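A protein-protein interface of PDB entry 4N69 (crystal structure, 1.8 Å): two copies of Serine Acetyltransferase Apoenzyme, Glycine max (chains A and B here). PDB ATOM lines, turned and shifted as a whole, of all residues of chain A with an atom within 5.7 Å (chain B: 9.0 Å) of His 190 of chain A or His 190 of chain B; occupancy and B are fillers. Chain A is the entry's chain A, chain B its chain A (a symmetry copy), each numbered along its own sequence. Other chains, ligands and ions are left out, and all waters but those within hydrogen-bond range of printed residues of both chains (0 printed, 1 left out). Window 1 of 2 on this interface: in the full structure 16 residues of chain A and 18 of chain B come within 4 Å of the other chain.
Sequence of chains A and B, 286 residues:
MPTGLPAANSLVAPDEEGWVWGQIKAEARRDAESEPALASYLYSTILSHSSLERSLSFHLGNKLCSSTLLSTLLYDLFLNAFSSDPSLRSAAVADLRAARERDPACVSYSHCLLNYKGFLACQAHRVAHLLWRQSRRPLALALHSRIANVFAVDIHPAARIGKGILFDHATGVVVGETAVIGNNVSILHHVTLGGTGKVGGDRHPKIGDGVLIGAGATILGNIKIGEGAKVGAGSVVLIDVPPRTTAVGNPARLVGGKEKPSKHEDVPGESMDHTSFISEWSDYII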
ATOM      1  N   ASP A 168     -25.560   2.055   4.397  1.00  0.00           N
ATOM      2  CA  ASP A 168     -26.109   0.728   4.347  1.00  0.00           C
ATOM      3  C   ASP A 168     -25.775   0.090   3.022  1.00  0.00           C
ATOM      4  O   ASP A 168     -26.302   0.498   1.986  1.00  0.00           O
ATOM      5  CB  ASP A 168     -27.611   0.765   4.549  1.00  0.00           C
ATOM      6  CG  ASP A 168     -28.233  -0.576   4.365  1.00  0.00           C
ATOM      7  OD1 ASP A 168     -27.932  -1.474   5.180  1.00  0.00           O
ATOM      8  OD2 ASP A 168     -29.017  -0.739   3.409  1.00  0.00           O
ATOM      9  N   HIS A 169     -24.906  -0.915   3.070  1.00  0.00           N
ATOM     10  CA  HIS A 169     -24.374  -1.544   1.867  1.00  0.00           C
ATOM     11  C   HIS A 169     -23.766  -0.443   1.016  1.00  0.00           C
ATOM     12  O   HIS A 169     -24.286  -0.060  -0.033  1.00  0.00           O
ATOM     13  CB  HIS A 169     -25.460  -2.325   1.123  1.00  0.00           C
ATOM     14  CG  HIS A 169     -26.234  -3.256   2.006  1.00  0.00           C
ATOM     15  ND1 HIS A 169     -27.504  -2.971   2.460  1.00  0.00           N
ATOM     16  CD2 HIS A 169     -25.905  -4.456   2.540  1.00  0.00           C
ATOM     17  CE1 HIS A 169     -27.931  -3.963   3.221  1.00  0.00           C
ATOM     18  NE2 HIS A 169     -26.979  -4.877   3.286  1.00  0.00           N
ATOM     19  N   ALA A 170     -22.649   0.070   1.510  1.00  0.00           N
ATOM     20  CA  ALA A 170     -22.005   1.254   0.976  1.00  0.00           C
ATOM     21  C   ALA A 170     -21.517   1.072  -0.444  1.00  0.00           C
ATOM     22  O   ALA A 170     -21.226   2.049  -1.132  1.00  0.00           O
ATOM     23  CB  ALA A 170     -20.846   1.644   1.870  1.00  0.00           C
ATOM     24  N   THR A 171     -21.411  -0.178  -0.872  1.00  0.00           N
ATOM     25  CA  THR A 171     -20.870  -0.472  -2.189  1.00  0.00           C
ATOM     26  C   THR A 171     -21.555   0.379  -3.251  1.00  0.00           C
ATOM     27  O   THR A 171     -22.781   0.442  -3.316  1.00  0.00           O
ATOM     28  CB  THR A 171     -21.023  -1.968  -2.549  1.00  0.00           C
ATOM     29  OG1 THR A 171     -20.440  -2.777  -1.519  1.00  0.00           O
ATOM     30  CG2 THR A 171     -20.344  -2.271  -3.874  1.00  0.00           C
ATOM     31  N   GLY A 172     -20.753   1.074  -4.043  1.00  0.00           N
ATOM     32  CA  GLY A 172     -21.265   1.830  -5.165  1.00  0.00           C
ATOM     33  C   GLY A 172     -21.832   3.185  -4.807  1.00  0.00           C
ATOM     34  O   GLY A 172     -22.405   3.852  -5.674  1.00  0.00           O
ATOM     35  N   VAL A 173     -21.669   3.612  -3.556  1.00  0.00           N
ATOM     36  CA  VAL A 173     -22.066   4.971  -3.183  1.00  0.00           C
ATOM     37  C   VAL A 173     -21.172   5.979  -3.897  1.00  0.00           C
ATOM     38  O   VAL A 173     -19.948   5.803  -3.947  1.00  0.00           O
ATOM     39  CB  VAL A 173     -21.998   5.202  -1.659  1.00  0.00           C
ATOM     40  CG1 VAL A 173     -22.080   6.681  -1.334  1.00  0.00           C
ATOM     41  CG2 VAL A 173     -23.142   4.486  -0.971  1.00  0.00           C
ATOM     42  N   LEU A 188     -28.407   4.887   1.701  1.00  0.00           N
ATOM     43  CA  LEU A 188     -28.497   3.446   1.527  1.00  0.00           C
ATOM     44  C   LEU A 188     -27.730   3.001   0.286  1.00  0.00           C
ATOM     45  O   LEU A 188     -26.993   3.781  -0.315  1.00  0.00           O
ATOM     46  CB  LEU A 188     -29.956   3.000   1.466  1.00  0.00           C
ATOM     47  CG  LEU A 188     -30.780   3.411   2.702  1.00  0.00           C
ATOM     48  CD1 LEU A 188     -32.075   2.613   2.810  1.00  0.00           C
ATOM     49  CD2 LEU A 188     -29.977   3.308   3.985  1.00  0.00           C
ATOM     50  N   HIS A 189     -27.907   1.736  -0.077  1.00  0.00           N
ATOM     51  CA  HIS A 189     -27.140   1.113  -1.143  1.00  0.00           C
ATOM     52  C   HIS A 189     -27.307   1.809  -2.490  1.00  0.00           C
ATOM     53  O   HIS A 189     -28.424   2.165  -2.881  1.00  0.00           O
ATOM     54  CB  HIS A 189     -27.548  -0.354  -1.272  1.00  0.00           C
ATOM     55  CG  HIS A 189     -26.797  -1.090  -2.332  1.00  0.00           C
ATOM     56  ND1 HIS A 189     -25.425  -1.015  -2.454  1.00  0.00           N
ATOM     57  CD2 HIS A 189     -27.221  -1.908  -3.323  1.00  0.00           C
ATOM     58  CE1 HIS A 189     -25.036  -1.763  -3.472  1.00  0.00           C
ATOM     59  NE2 HIS A 189     -26.106  -2.313  -4.018  1.00  0.00           N
ATOM     60  N   HIS A 190     -26.184   1.997  -3.187  1.00  0.00           N
ATOM     61  CA  HIS A 190     -26.171   2.500  -4.558  1.00  0.00           C
ATOM     62  C   HIS A 190     -26.811   3.862  -4.710  1.00  0.00           C
ATOM     63  O   HIS A 190     -27.512   4.119  -5.690  1.00  0.00           O
ATOM     64  CB  HIS A 190     -26.855   1.505  -5.495  1.00  0.00           C
ATOM     65  CG  HIS A 190     -25.942   0.426  -5.976  1.00  0.00           C
ATOM     66  ND1 HIS A 190     -26.382  -0.664  -6.694  1.00  0.00           N
ATOM     67  CD2 HIS A 190     -24.603   0.278  -5.846  1.00  0.00           C
ATOM     68  CE1 HIS A 190     -25.353  -1.443  -6.981  1.00  0.00           C
ATOM     69  NE2 HIS A 190     -24.262  -0.894  -6.474  1.00  0.00           N
ATOM     70  N   VAL A 191     -26.571   4.734  -3.739  1.00  0.00           N
ATOM     71  CA  VAL A 191     -27.040   6.108  -3.856  1.00  0.00           C
ATOM     72  C   VAL A 191     -26.000   6.901  -4.632  1.00  0.00           C
ATOM     73  O   VAL A 191     -24.790   6.725  -4.441  1.00  0.00           O
ATOM     74  CB  VAL A 191     -27.310   6.749  -2.481  1.00  0.00           C
ATOM     75  CG1 VAL A 191     -27.359   8.271  -2.581  1.00  0.00           C
ATOM     76  CG2 VAL A 191     -28.636   6.226  -1.916  1.00  0.00           C
ATOM     77  N   THR A 192     -26.486   7.742  -5.536  1.00  0.00           N
ATOM     78  CA  THR A 192     -25.635   8.652  -6.278  1.00  0.00           C
ATOM     79  C   THR A 192     -26.047  10.084  -5.990  1.00  0.00           C
ATOM     80  O   THR A 192     -27.187  10.483  -6.244  1.00  0.00           O
ATOM     81  CB  THR A 192     -25.713   8.392  -7.783  1.00  0.00           C
ATOM     82  OG1 THR A 192     -25.309   7.047  -8.053  1.00  0.00           O
ATOM     83  CG2 THR A 192     -24.808   9.355  -8.534  1.00  0.00           C
ATOM     84  N   ALA A 215     -32.457   3.067  -1.216  1.00  0.00           N
ATOM     85  CA  ALA A 215     -31.536   2.328  -2.075  1.00  0.00           C
ATOM     86  C   ALA A 215     -31.734   2.658  -3.555  1.00  0.00           C
ATOM     87  O   ALA A 215     -32.865   2.755  -4.045  1.00  0.00           O
ATOM     88  CB  ALA A 215     -31.682   0.836  -1.844  1.00  0.00           C
ATOM     89  N   GLY A 216     -30.613   2.858  -4.244  1.00  0.00           N
ATOM     90  CA  GLY A 216     -30.598   3.096  -5.675  1.00  0.00           C
ATOM     91  C   GLY A 216     -31.049   4.477  -6.106  1.00  0.00           C
ATOM     92  O   GLY A 216     -31.174   4.734  -7.300  1.00  0.00           O
ATOM     93  N   ALA A 217     -31.300   5.369  -5.150  1.00  0.00           N
ATOM     94  CA  ALA A 217     -31.757   6.708  -5.496  1.00  0.00           C
ATOM     95  C   ALA A 217     -30.623   7.488  -6.139  1.00  0.00           C
ATOM     96  O   ALA A 217     -29.474   7.389  -5.710  1.00  0.00           O
ATOM     97  CB  ALA A 217     -32.283   7.442  -4.267  1.00  0.00           C
ATOM     98  N   THR A 218     -30.950   8.246  -7.179  1.00  0.00           N
ATOM     99  CA  THR A 218     -29.992   9.156  -7.794  1.00  0.00           C
ATOM    100  C   THR A 218     -30.521  10.569  -7.654  1.00  0.00           C
ATOM    101  O   THR A 218     -31.669  10.864  -8.006  1.00  0.00           O
ATOM    102  CB  THR A 218     -29.755   8.856  -9.282  1.00  0.00           C
ATOM    103  OG1 THR A 218     -30.845   9.371 -10.050  1.00  0.00           O
ATOM    104  CG2 THR A 218     -29.660   7.370  -9.519  1.00  0.00           C
ATOM    105  N   ALA B 152     -17.302  -8.701  -5.451  1.00  0.00           N
ATOM    106  CA  ALA B 152     -18.364  -7.702  -5.538  1.00  0.00           C
ATOM    107  C   ALA B 152     -19.742  -8.341  -5.354  1.00  0.00           C
ATOM    108  O   ALA B 152     -20.706  -8.012  -6.047  1.00  0.00           O
ATOM    109  CB  ALA B 152     -18.278  -6.965  -6.854  1.00  0.00           C
ATOM    110  N   PHE B 167     -25.667 -16.341 -11.566  1.00  0.00           N
ATOM    111  CA  PHE B 167     -25.401 -14.917 -11.517  1.00  0.00           C
ATOM    112  C   PHE B 167     -25.091 -14.407 -12.904  1.00  0.00           C
ATOM    113  O   PHE B 167     -24.740 -15.164 -13.807  1.00  0.00           O
ATOM    114  CB  PHE B 167     -24.258 -14.609 -10.560  1.00  0.00           C
ATOM    115  CG  PHE B 167     -24.588 -14.943  -9.152  1.00  0.00           C
ATOM    116  CD1 PHE B 167     -25.181 -14.004  -8.333  1.00  0.00           C
ATOM    117  CD2 PHE B 167     -24.376 -16.220  -8.664  1.00  0.00           C
ATOM    118  CE1 PHE B 167     -25.525 -14.313  -7.046  1.00  0.00           C
ATOM    119  CE2 PHE B 167     -24.719 -16.530  -7.368  1.00  0.00           C
ATOM    120  CZ  PHE B 167     -25.292 -15.572  -6.561  1.00  0.00           C
ATOM    121  N   ASP B 168     -25.251 -13.109 -13.073  1.00  0.00           N
ATOM    122  CA  ASP B 168     -24.829 -12.478 -14.293  1.00  0.00           C
ATOM    123  C   ASP B 168     -24.325 -11.088 -13.998  1.00  0.00           C
ATOM    124  O   ASP B 168     -25.109 -10.204 -13.647  1.00  0.00           O
ATOM    125  CB  ASP B 168     -25.972 -12.423 -15.287  1.00  0.00           C
ATOM    126  CG  ASP B 168     -25.613 -11.652 -16.511  1.00  0.00           C
ATOM    127  OD1 ASP B 168     -24.714 -12.114 -17.247  1.00  0.00           O
ATOM    128  OD2 ASP B 168     -26.219 -10.586 -16.739  1.00  0.00           O
ATOM    129  N   HIS B 169     -23.017 -10.905 -14.151  1.00  0.00           N
ATOM    130  CA  HIS B 169     -22.354  -9.664 -13.773  1.00  0.00           C
ATOM    131  C   HIS B 169     -22.693  -9.397 -12.317  1.00  0.00           C
ATOM    132  O   HIS B 169     -23.457  -8.493 -11.975  1.00  0.00           O
ATOM    133  CB  HIS B 169     -22.770  -8.510 -14.690  1.00  0.00           C
ATOM    134  CG  HIS B 169     -22.662  -8.840 -16.148  1.00  0.00           C
ATOM    135  ND1 HIS B 169     -23.756  -9.147 -16.928  1.00  0.00           N
ATOM    136  CD2 HIS B 169     -21.583  -8.938 -16.960  1.00  0.00           C
ATOM    137  CE1 HIS B 169     -23.359  -9.401 -18.161  1.00  0.00           C
ATOM    138  NE2 HIS B 169     -22.044  -9.282 -18.208  1.00  0.00           N
ATOM    139  N   ALA B 170     -22.111 -10.227 -11.465  1.00  0.00           N
ATOM    140  CA  ALA B 170     -22.439 -10.289 -10.053  1.00  0.00           C
ATOM    141  C   ALA B 170     -22.120  -9.006  -9.317  1.00  0.00           C
ATOM    142  O   ALA B 170     -22.603  -8.789  -8.207  1.00  0.00           O
ATOM    143  CB  ALA B 170     -21.699 -11.445  -9.414  1.00  0.00           C
ATOM    144  N   THR B 171     -21.293  -8.169  -9.927  1.00  0.00           N
ATOM    145  CA  THR B 171     -20.849  -6.948  -9.273  1.00  0.00           C
ATOM    146  C   THR B 171     -22.038  -6.179  -8.714  1.00  0.00           C
ATOM    147  O   THR B 171     -23.020  -5.936  -9.413  1.00  0.00           O
ATOM    148  CB  THR B 171     -20.055  -6.039 -10.239  1.00  0.00           C
ATOM    149  OG1 THR B 171     -18.973  -6.778 -10.822  1.00  0.00           O
ATOM    150  CG2 THR B 171     -19.502  -4.831  -9.502  1.00  0.00           C
ATOM    151  N   GLY B 172     -21.965  -5.849  -7.433  1.00  0.00           N
ATOM    152  CA  GLY B 172     -22.970  -5.019  -6.806  1.00  0.00           C
ATOM    153  C   GLY B 172     -24.223  -5.753  -6.385  1.00  0.00           C
ATOM    154  O   GLY B 172     -25.188  -5.112  -5.955  1.00  0.00           O
ATOM    155  N   VAL B 173     -24.223  -7.081  -6.483  1.00  0.00           N
ATOM    156  CA  VAL B 173     -25.347  -7.859  -5.960  1.00  0.00           C
ATOM    157  C   VAL B 173     -25.394  -7.733  -4.440  1.00  0.00           C
ATOM    158  O   VAL B 173     -24.356  -7.828  -3.774  1.00  0.00           O
ATOM    159  CB  VAL B 173     -25.262  -9.348  -6.355  1.00  0.00           C
ATOM    160  CG1 VAL B 173     -26.230 -10.180  -5.534  1.00  0.00           C
ATOM    161  CG2 VAL B 173     -25.595  -9.517  -7.823  1.00  0.00           C
ATOM    162  N   VAL B 174     -26.587  -7.484  -3.905  1.00  0.00           N
ATOM    163  CA  VAL B 174     -26.795  -7.397  -2.461  1.00  0.00           C
ATOM    164  C   VAL B 174     -27.944  -8.300  -2.030  1.00  0.00           C
ATOM    165  O   VAL B 174     -29.050  -8.210  -2.561  1.00  0.00           O
ATOM    166  CB  VAL B 174     -27.094  -5.955  -2.010  1.00  0.00           C
ATOM    167  CG1 VAL B 174     -27.563  -5.941  -0.568  1.00  0.00           C
ATOM    168  CG2 VAL B 174     -25.868  -5.056  -2.196  1.00  0.00           C
ATOM    169  N   VAL B 175     -27.670  -9.189  -1.082  1.00  0.00           N
ATOM    170  CA  VAL B 175     -28.684 -10.089  -0.532  1.00  0.00           C
ATOM    171  C   VAL B 175     -28.643  -9.986   0.988  1.00  0.00           C
ATOM    172  O   VAL B 175     -27.650 -10.343   1.621  1.00  0.00           O
ATOM    173  CB  VAL B 175     -28.472 -11.560  -0.956  1.00  0.00           C
ATOM    174  CG1 VAL B 175     -29.534 -12.465  -0.309  1.00  0.00           C
ATOM    175  CG2 VAL B 175     -28.497 -11.696  -2.473  1.00  0.00           C
ATOM    176  N   ILE B 187     -30.128 -14.358 -10.910  1.00  0.00           N
ATOM    177  CA  ILE B 187     -29.992 -13.023 -10.344  1.00  0.00           C
ATOM    178  C   ILE B 187     -29.028 -12.223 -11.202  1.00  0.00           C
ATOM    179  O   ILE B 187     -27.830 -12.519 -11.242  1.00  0.00           O
ATOM    180  CB  ILE B 187     -29.472 -13.074  -8.900  1.00  0.00           C
ATOM    181  CG1 ILE B 187     -30.370 -13.965  -8.031  1.00  0.00           C
ATOM    182  CG2 ILE B 187     -29.343 -11.675  -8.320  1.00  0.00           C
ATOM    183  CD1 ILE B 187     -29.601 -14.696  -6.940  1.00  0.00           C
ATOM    184  N   LEU B 188     -29.543 -11.217 -11.892  1.00  0.00           N
ATOM    185  CA  LEU B 188     -28.714 -10.508 -12.853  1.00  0.00           C
ATOM    186  C   LEU B 188     -27.993  -9.340 -12.190  1.00  0.00           C
ATOM    187  O   LEU B 188     -28.000  -9.205 -10.966  1.00  0.00           O
ATOM    188  CB  LEU B 188     -29.548 -10.041 -14.044  1.00  0.00           C
ATOM    189  CG  LEU B 188     -30.290 -11.183 -14.764  1.00  0.00           C
ATOM    190  CD1 LEU B 188     -30.755 -10.767 -16.157  1.00  0.00           C
ATOM    191  CD2 LEU B 188     -29.461 -12.452 -14.831  1.00  0.00           C
ATOM    192  N   HIS B 189     -27.364  -8.508 -13.012  1.00  0.00           N
ATOM    193  CA  HIS B 189     -26.509  -7.435 -12.536  1.00  0.00           C
ATOM    194  C   HIS B 189     -27.240  -6.435 -11.646  1.00  0.00           C
ATOM    195  O   HIS B 189     -28.363  -6.021 -11.952  1.00  0.00           O
ATOM    196  CB  HIS B 189     -25.899  -6.702 -13.732  1.00  0.00           C
ATOM    197  CG  HIS B 189     -24.985  -5.589 -13.346  1.00  0.00           C
ATOM    198  ND1 HIS B 189     -24.002  -5.736 -12.389  1.00  0.00           N
ATOM    199  CD2 HIS B 189     -24.903  -4.308 -13.777  1.00  0.00           C
ATOM    200  CE1 HIS B 189     -23.349  -4.595 -12.253  1.00  0.00           C
ATOM    201  NE2 HIS B 189     -23.878  -3.711 -13.081  1.00  0.00           N
ATOM    202  N   HIS B 190     -26.587  -6.056 -10.544  1.00  0.00           N
ATOM    203  CA  HIS B 190     -27.059  -4.993  -9.662  1.00  0.00           C
ATOM    204  C   HIS B 190     -28.434  -5.252  -9.083  1.00  0.00           C
ATOM    205  O   HIS B 190     -29.247  -4.335  -8.966  1.00  0.00           O
ATOM    206  CB  HIS B 190     -27.058  -3.653 -10.396  1.00  0.00           C
ATOM    207  CG  HIS B 190     -25.731  -2.968 -10.366  1.00  0.00           C
ATOM    208  ND1 HIS B 190     -25.457  -1.833 -11.096  1.00  0.00           N
ATOM    209  CD2 HIS B 190     -24.602  -3.258  -9.678  1.00  0.00           C
ATOM    210  CE1 HIS B 190     -24.211  -1.456 -10.865  1.00  0.00           C
ATOM    211  NE2 HIS B 190     -23.670  -2.306 -10.011  1.00  0.00           N
ATOM    212  N   VAL B 191     -28.692  -6.502  -8.723  1.00  0.00           N
ATOM    213  CA  VAL B 191     -29.939  -6.827  -8.043  1.00  0.00           C
ATOM    214  C   VAL B 191     -29.745  -6.588  -6.554  1.00  0.00           C
ATOM    215  O   VAL B 191     -28.689  -6.902  -5.990  1.00  0.00           O
ATOM    216  CB  VAL B 191     -30.390  -8.275  -8.316  1.00  0.00           C
ATOM    217  CG1 VAL B 191     -31.410  -8.741  -7.279  1.00  0.00           C
ATOM    218  CG2 VAL B 191     -30.999  -8.373  -9.720  1.00  0.00           C
ATOM    219  N   THR B 192     -30.757  -5.993  -5.938  1.00  0.00           N
ATOM    220  CA  THR B 192     -30.778  -5.796  -4.501  1.00  0.00           C
ATOM    221  C   THR B 192     -31.970  -6.522  -3.905  1.00  0.00           C
ATOM    222  O   THR B 192     -33.122  -6.246  -4.250  1.00  0.00           O
ATOM    223  CB  THR B 192     -30.849  -4.313  -4.138  1.00  0.00           C
ATOM    224  OG1 THR B 192     -29.716  -3.635  -4.689  1.00  0.00           O
ATOM    225  CG2 THR B 192     -30.864  -4.137  -2.629  1.00  0.00           C
ATOM    226  N   LEU B 193     -31.681  -7.476  -3.029  1.00  0.00           N
ATOM    227  CA  LEU B 193     -32.698  -8.117  -2.217  1.00  0.00           C
ATOM    228  C   LEU B 193     -32.476  -7.619  -0.799  1.00  0.00           C
ATOM    229  O   LEU B 193     -31.791  -8.261   0.002  1.00  0.00           O
ATOM    230  CB  LEU B 193     -32.594  -9.634  -2.307  1.00  0.00           C
ATOM    231  CG  LEU B 193     -32.611 -10.190  -3.722  1.00  0.00           C
ATOM    232  CD1 LEU B 193     -32.432 -11.696  -3.706  1.00  0.00           C
ATOM    233  CD2 LEU B 193     -33.932  -9.810  -4.423  1.00  0.00           C
ATOM    234  N   ILE B 213     -34.691 -12.677 -11.966  1.00  0.00           N
ATOM    235  CA  ILE B 213     -34.670 -11.275 -11.549  1.00  0.00           C
ATOM    236  C   ILE B 213     -33.756 -10.453 -12.458  1.00  0.00           C
ATOM    237  O   ILE B 213     -32.541 -10.657 -12.480  1.00  0.00           O
ATOM    238  CB  ILE B 213     -34.211 -11.135 -10.083  1.00  0.00           C
ATOM    239  CG1 ILE B 213     -34.974 -12.128  -9.201  1.00  0.00           C
ATOM    240  CG2 ILE B 213     -34.390  -9.686  -9.587  1.00  0.00           C
ATOM    241  CD1 ILE B 213     -34.573 -12.090  -7.738  1.00  0.00           C
ATOM    242  N   GLY B 214     -34.354  -9.526 -13.204  1.00  0.00           N
ATOM    243  CA  GLY B 214     -33.643  -8.735 -14.195  1.00  0.00           C
ATOM    244  C   GLY B 214     -32.669  -7.712 -13.641  1.00  0.00           C
ATOM    245  O   GLY B 214     -32.695  -7.381 -12.451  1.00  0.00           O
ATOM    246  N   ALA B 215     -31.811  -7.195 -14.517  1.00  0.00           N
ATOM    247  CA  ALA B 215     -30.741  -6.291 -14.105  1.00  0.00           C
ATOM    248  C   ALA B 215     -31.277  -5.030 -13.429  1.00  0.00           C
ATOM    249  O   ALA B 215     -32.258  -4.427 -13.881  1.00  0.00           O
ATOM    250  CB  ALA B 215     -29.873  -5.924 -15.294  1.00  0.00           C
ATOM    251  N   GLY B 216     -30.633  -4.663 -12.324  1.00  0.00           N
ATOM    252  CA  GLY B 216     -30.942  -3.447 -11.595  1.00  0.00           C
ATOM    253  C   GLY B 216     -32.217  -3.491 -10.777  1.00  0.00           C
ATOM    254  O   GLY B 216     -32.618  -2.475 -10.216  1.00  0.00           O
ATOM    255  N   ALA B 217     -32.864  -4.652 -10.705  1.00  0.00           N
ATOM    256  CA  ALA B 217     -34.106  -4.756  -9.951  1.00  0.00           C
ATOM    257  C   ALA B 217     -33.817  -4.650  -8.465  1.00  0.00           C
ATOM    258  O   ALA B 217     -32.828  -5.199  -7.979  1.00  0.00           O
ATOM    259  CB  ALA B 217     -34.829  -6.062 -10.265  1.00  0.00           C
ATOM    260  N   THR B 218     -34.672  -3.927  -7.752  1.00  0.00           N
ATOM    261  CA  THR B 218     -34.595  -3.864  -6.298  1.00  0.00           C
ATOM    262  C   THR B 218     -35.883  -4.428  -5.729  1.00  0.00           C
ATOM    263  O   THR B 218     -36.985  -4.022  -6.112  1.00  0.00           O
ATOM    264  CB  THR B 218     -34.400  -2.434  -5.771  1.00  0.00           C
ATOM    265  OG1 THR B 218     -35.649  -1.740  -5.806  1.00  0.00           O
ATOM    266  CG2 THR B 218     -33.409  -1.682  -6.622  1.00  0.00           C
ATOM    267  N   ILE B 219     -35.739  -5.386  -4.831  1.00  0.00           N
ATOM    268  CA  ILE B 219     -36.883  -5.994  -4.186  1.00  0.00           C
ATOM    269  C   ILE B 219     -36.727  -5.746  -2.693  1.00  0.00           C
ATOM    270  O   ILE B 219     -35.796  -6.247  -2.069  1.00  0.00           O
ATOM    271  CB  ILE B 219     -36.975  -7.496  -4.511  1.00  0.00           C
ATOM    272  CG1 ILE B 219     -36.908  -7.705  -6.029  1.00  0.00           C
ATOM    273  CG2 ILE B 219     -38.261  -8.079  -3.960  1.00  0.00           C
ATOM    274  CD1 ILE B 219     -36.978  -9.147  -6.463  1.00  0.00           C
ATOM    275  N   ALA B 233     -36.149  -5.833 -15.697  1.00  0.00           N
ATOM    276  CA  ALA B 233     -35.004  -4.993 -15.372  1.00  0.00           C
ATOM    277  C   ALA B 233     -35.452  -3.644 -14.829  1.00  0.00           C
ATOM    278  O   ALA B 233     -36.460  -3.091 -15.275  1.00  0.00           O
ATOM    279  CB  ALA B 233     -34.126  -4.806 -16.588  1.00  0.00           C
ATOM    280  N   GLY B 234     -34.714  -3.137 -13.844  1.00  0.00           N
ATOM    281  CA  GLY B 234     -34.941  -1.812 -13.307  1.00  0.00           C
ATOM    282  C   GLY B 234     -36.159  -1.684 -12.411  1.00  0.00           C
ATOM    283  O   GLY B 234     -36.488  -0.587 -11.974  1.00  0.00           O
ATOM    284  N   SER B 235     -36.832  -2.796 -12.131  1.00  0.00           N
ATOM    285  CA  SER B 235     -38.042  -2.744 -11.313  1.00  0.00           C
ATOM    286  C   SER B 235     -37.754  -2.423  -9.851  1.00  0.00           C
ATOM    287  O   SER B 235     -36.696  -2.765  -9.315  1.00  0.00           O
ATOM    288  CB  SER B 235     -38.809  -4.070 -11.392  1.00  0.00           C
ATOM    289  OG  SER B 235     -39.110  -4.408 -12.729  1.00  0.00           O
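A ring nitrogen (NE2) of His 189 of chain B is in hydrogen-bond range of a ring nitrogen (ND1) of His 190 of chain B, at 3.2 Å.
The backbone carbonyl oxygen of Val 191 of chain B lies within hydrogen-bond range of the backbone NH of Val 174 of chain B (3.0 Å).
O of Ala 152 of chain B is in hydrogen-bond range of N of Gly 172 of chain B (2.9 Å).
The backbone carbonyl oxygen (O) of Thr 192 of chain B lies within hydrogen-bond range of the backbone NH (N) of Ile 219 of chain B (2.8 Å).
A ring nitrogen (NE2) of His 189 of chain A sits at hydrogen-bond distance from a ring nitrogen (ND1) of His 190 of chain A (3.2 Å).
ND1 of His 169 of chain A is in hydrogen-bond range of OD2 of Asp 168 of chain A (2.9 Å).
Among the printed residues, pairs that only touch across the chains: His 169 of chain A with Val 174 of chain B, His 189 of chain A with Gly 172 of chain B, His 189 of chain A with Val 174 of chain B, His 189 of chain A with Thr 192 of chain B, His 190 of chain A with Gly 172 of chain B and His 190 of chain A with His 190 of chain B.
His 190 of chain B touches just one residue of chain A: His 190 (3.3 Å).
No residue of chain B comes within 4 Å of Gly 172 of chain A.
No residue of chain B comes within 4 Å of Val 191 of chain A.
No residue of chain B comes within 4 Å of Gly 216 of chain A.
Printed residues of chain A within 4 Å of Val 174 of chain B: His 169 and His 189.
Of the printed residues of chain B, His 169 of chain A touches Val 174 (3.8 Å).
Val 191 of chain B touches none of the printed residues of chain A.
The nearest residue of chain B that does not touch His 190 of chain A is Thr 192 of chain B (4.9 Å).
The nearest printed residue of chain A that does not touch Val 174 of chain B is Thr 171 of chain A (5.8 Å).
Hydrophobic or aromatic side chains of chain B within 4 Å of the printed part of chain A: Val 174 and His 190.
Of the 15 printed residues of chain A, 3 touch a printed residue of chain B.
Hydrophobic or aromatic side chains of chain A within 4 Å of the printed part of chain B: His 169, His 189 and His 190.
Among the printed residues, no Asp or Glu carboxylate lies within 4 Å of a Lys or Arg side-chain nitrogen of the other chain.
His 189 of chain A touches Gly 172 of chain B, but with the chains exchanged Gly 172 of chain A does not touch His 189 of chain B (9.8 Å).
His 189 of chain A touches Thr 192 of chain B, but with the chains exchanged Thr 192 of chain A does not touch His 189 of chain B (12.0 Å).
His 190 of chain A touches Gly 172 of chain B, but with the chains exchanged Gly 172 of chain A does not touch His 190 of chain B (6.8 Å).
His 190 of chain B touches its own counterpart, His 190 of chain A.
Of the 6 pairs that touch across the chains among the printed residues, 1 has its exchanged pair printed and touching as well.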
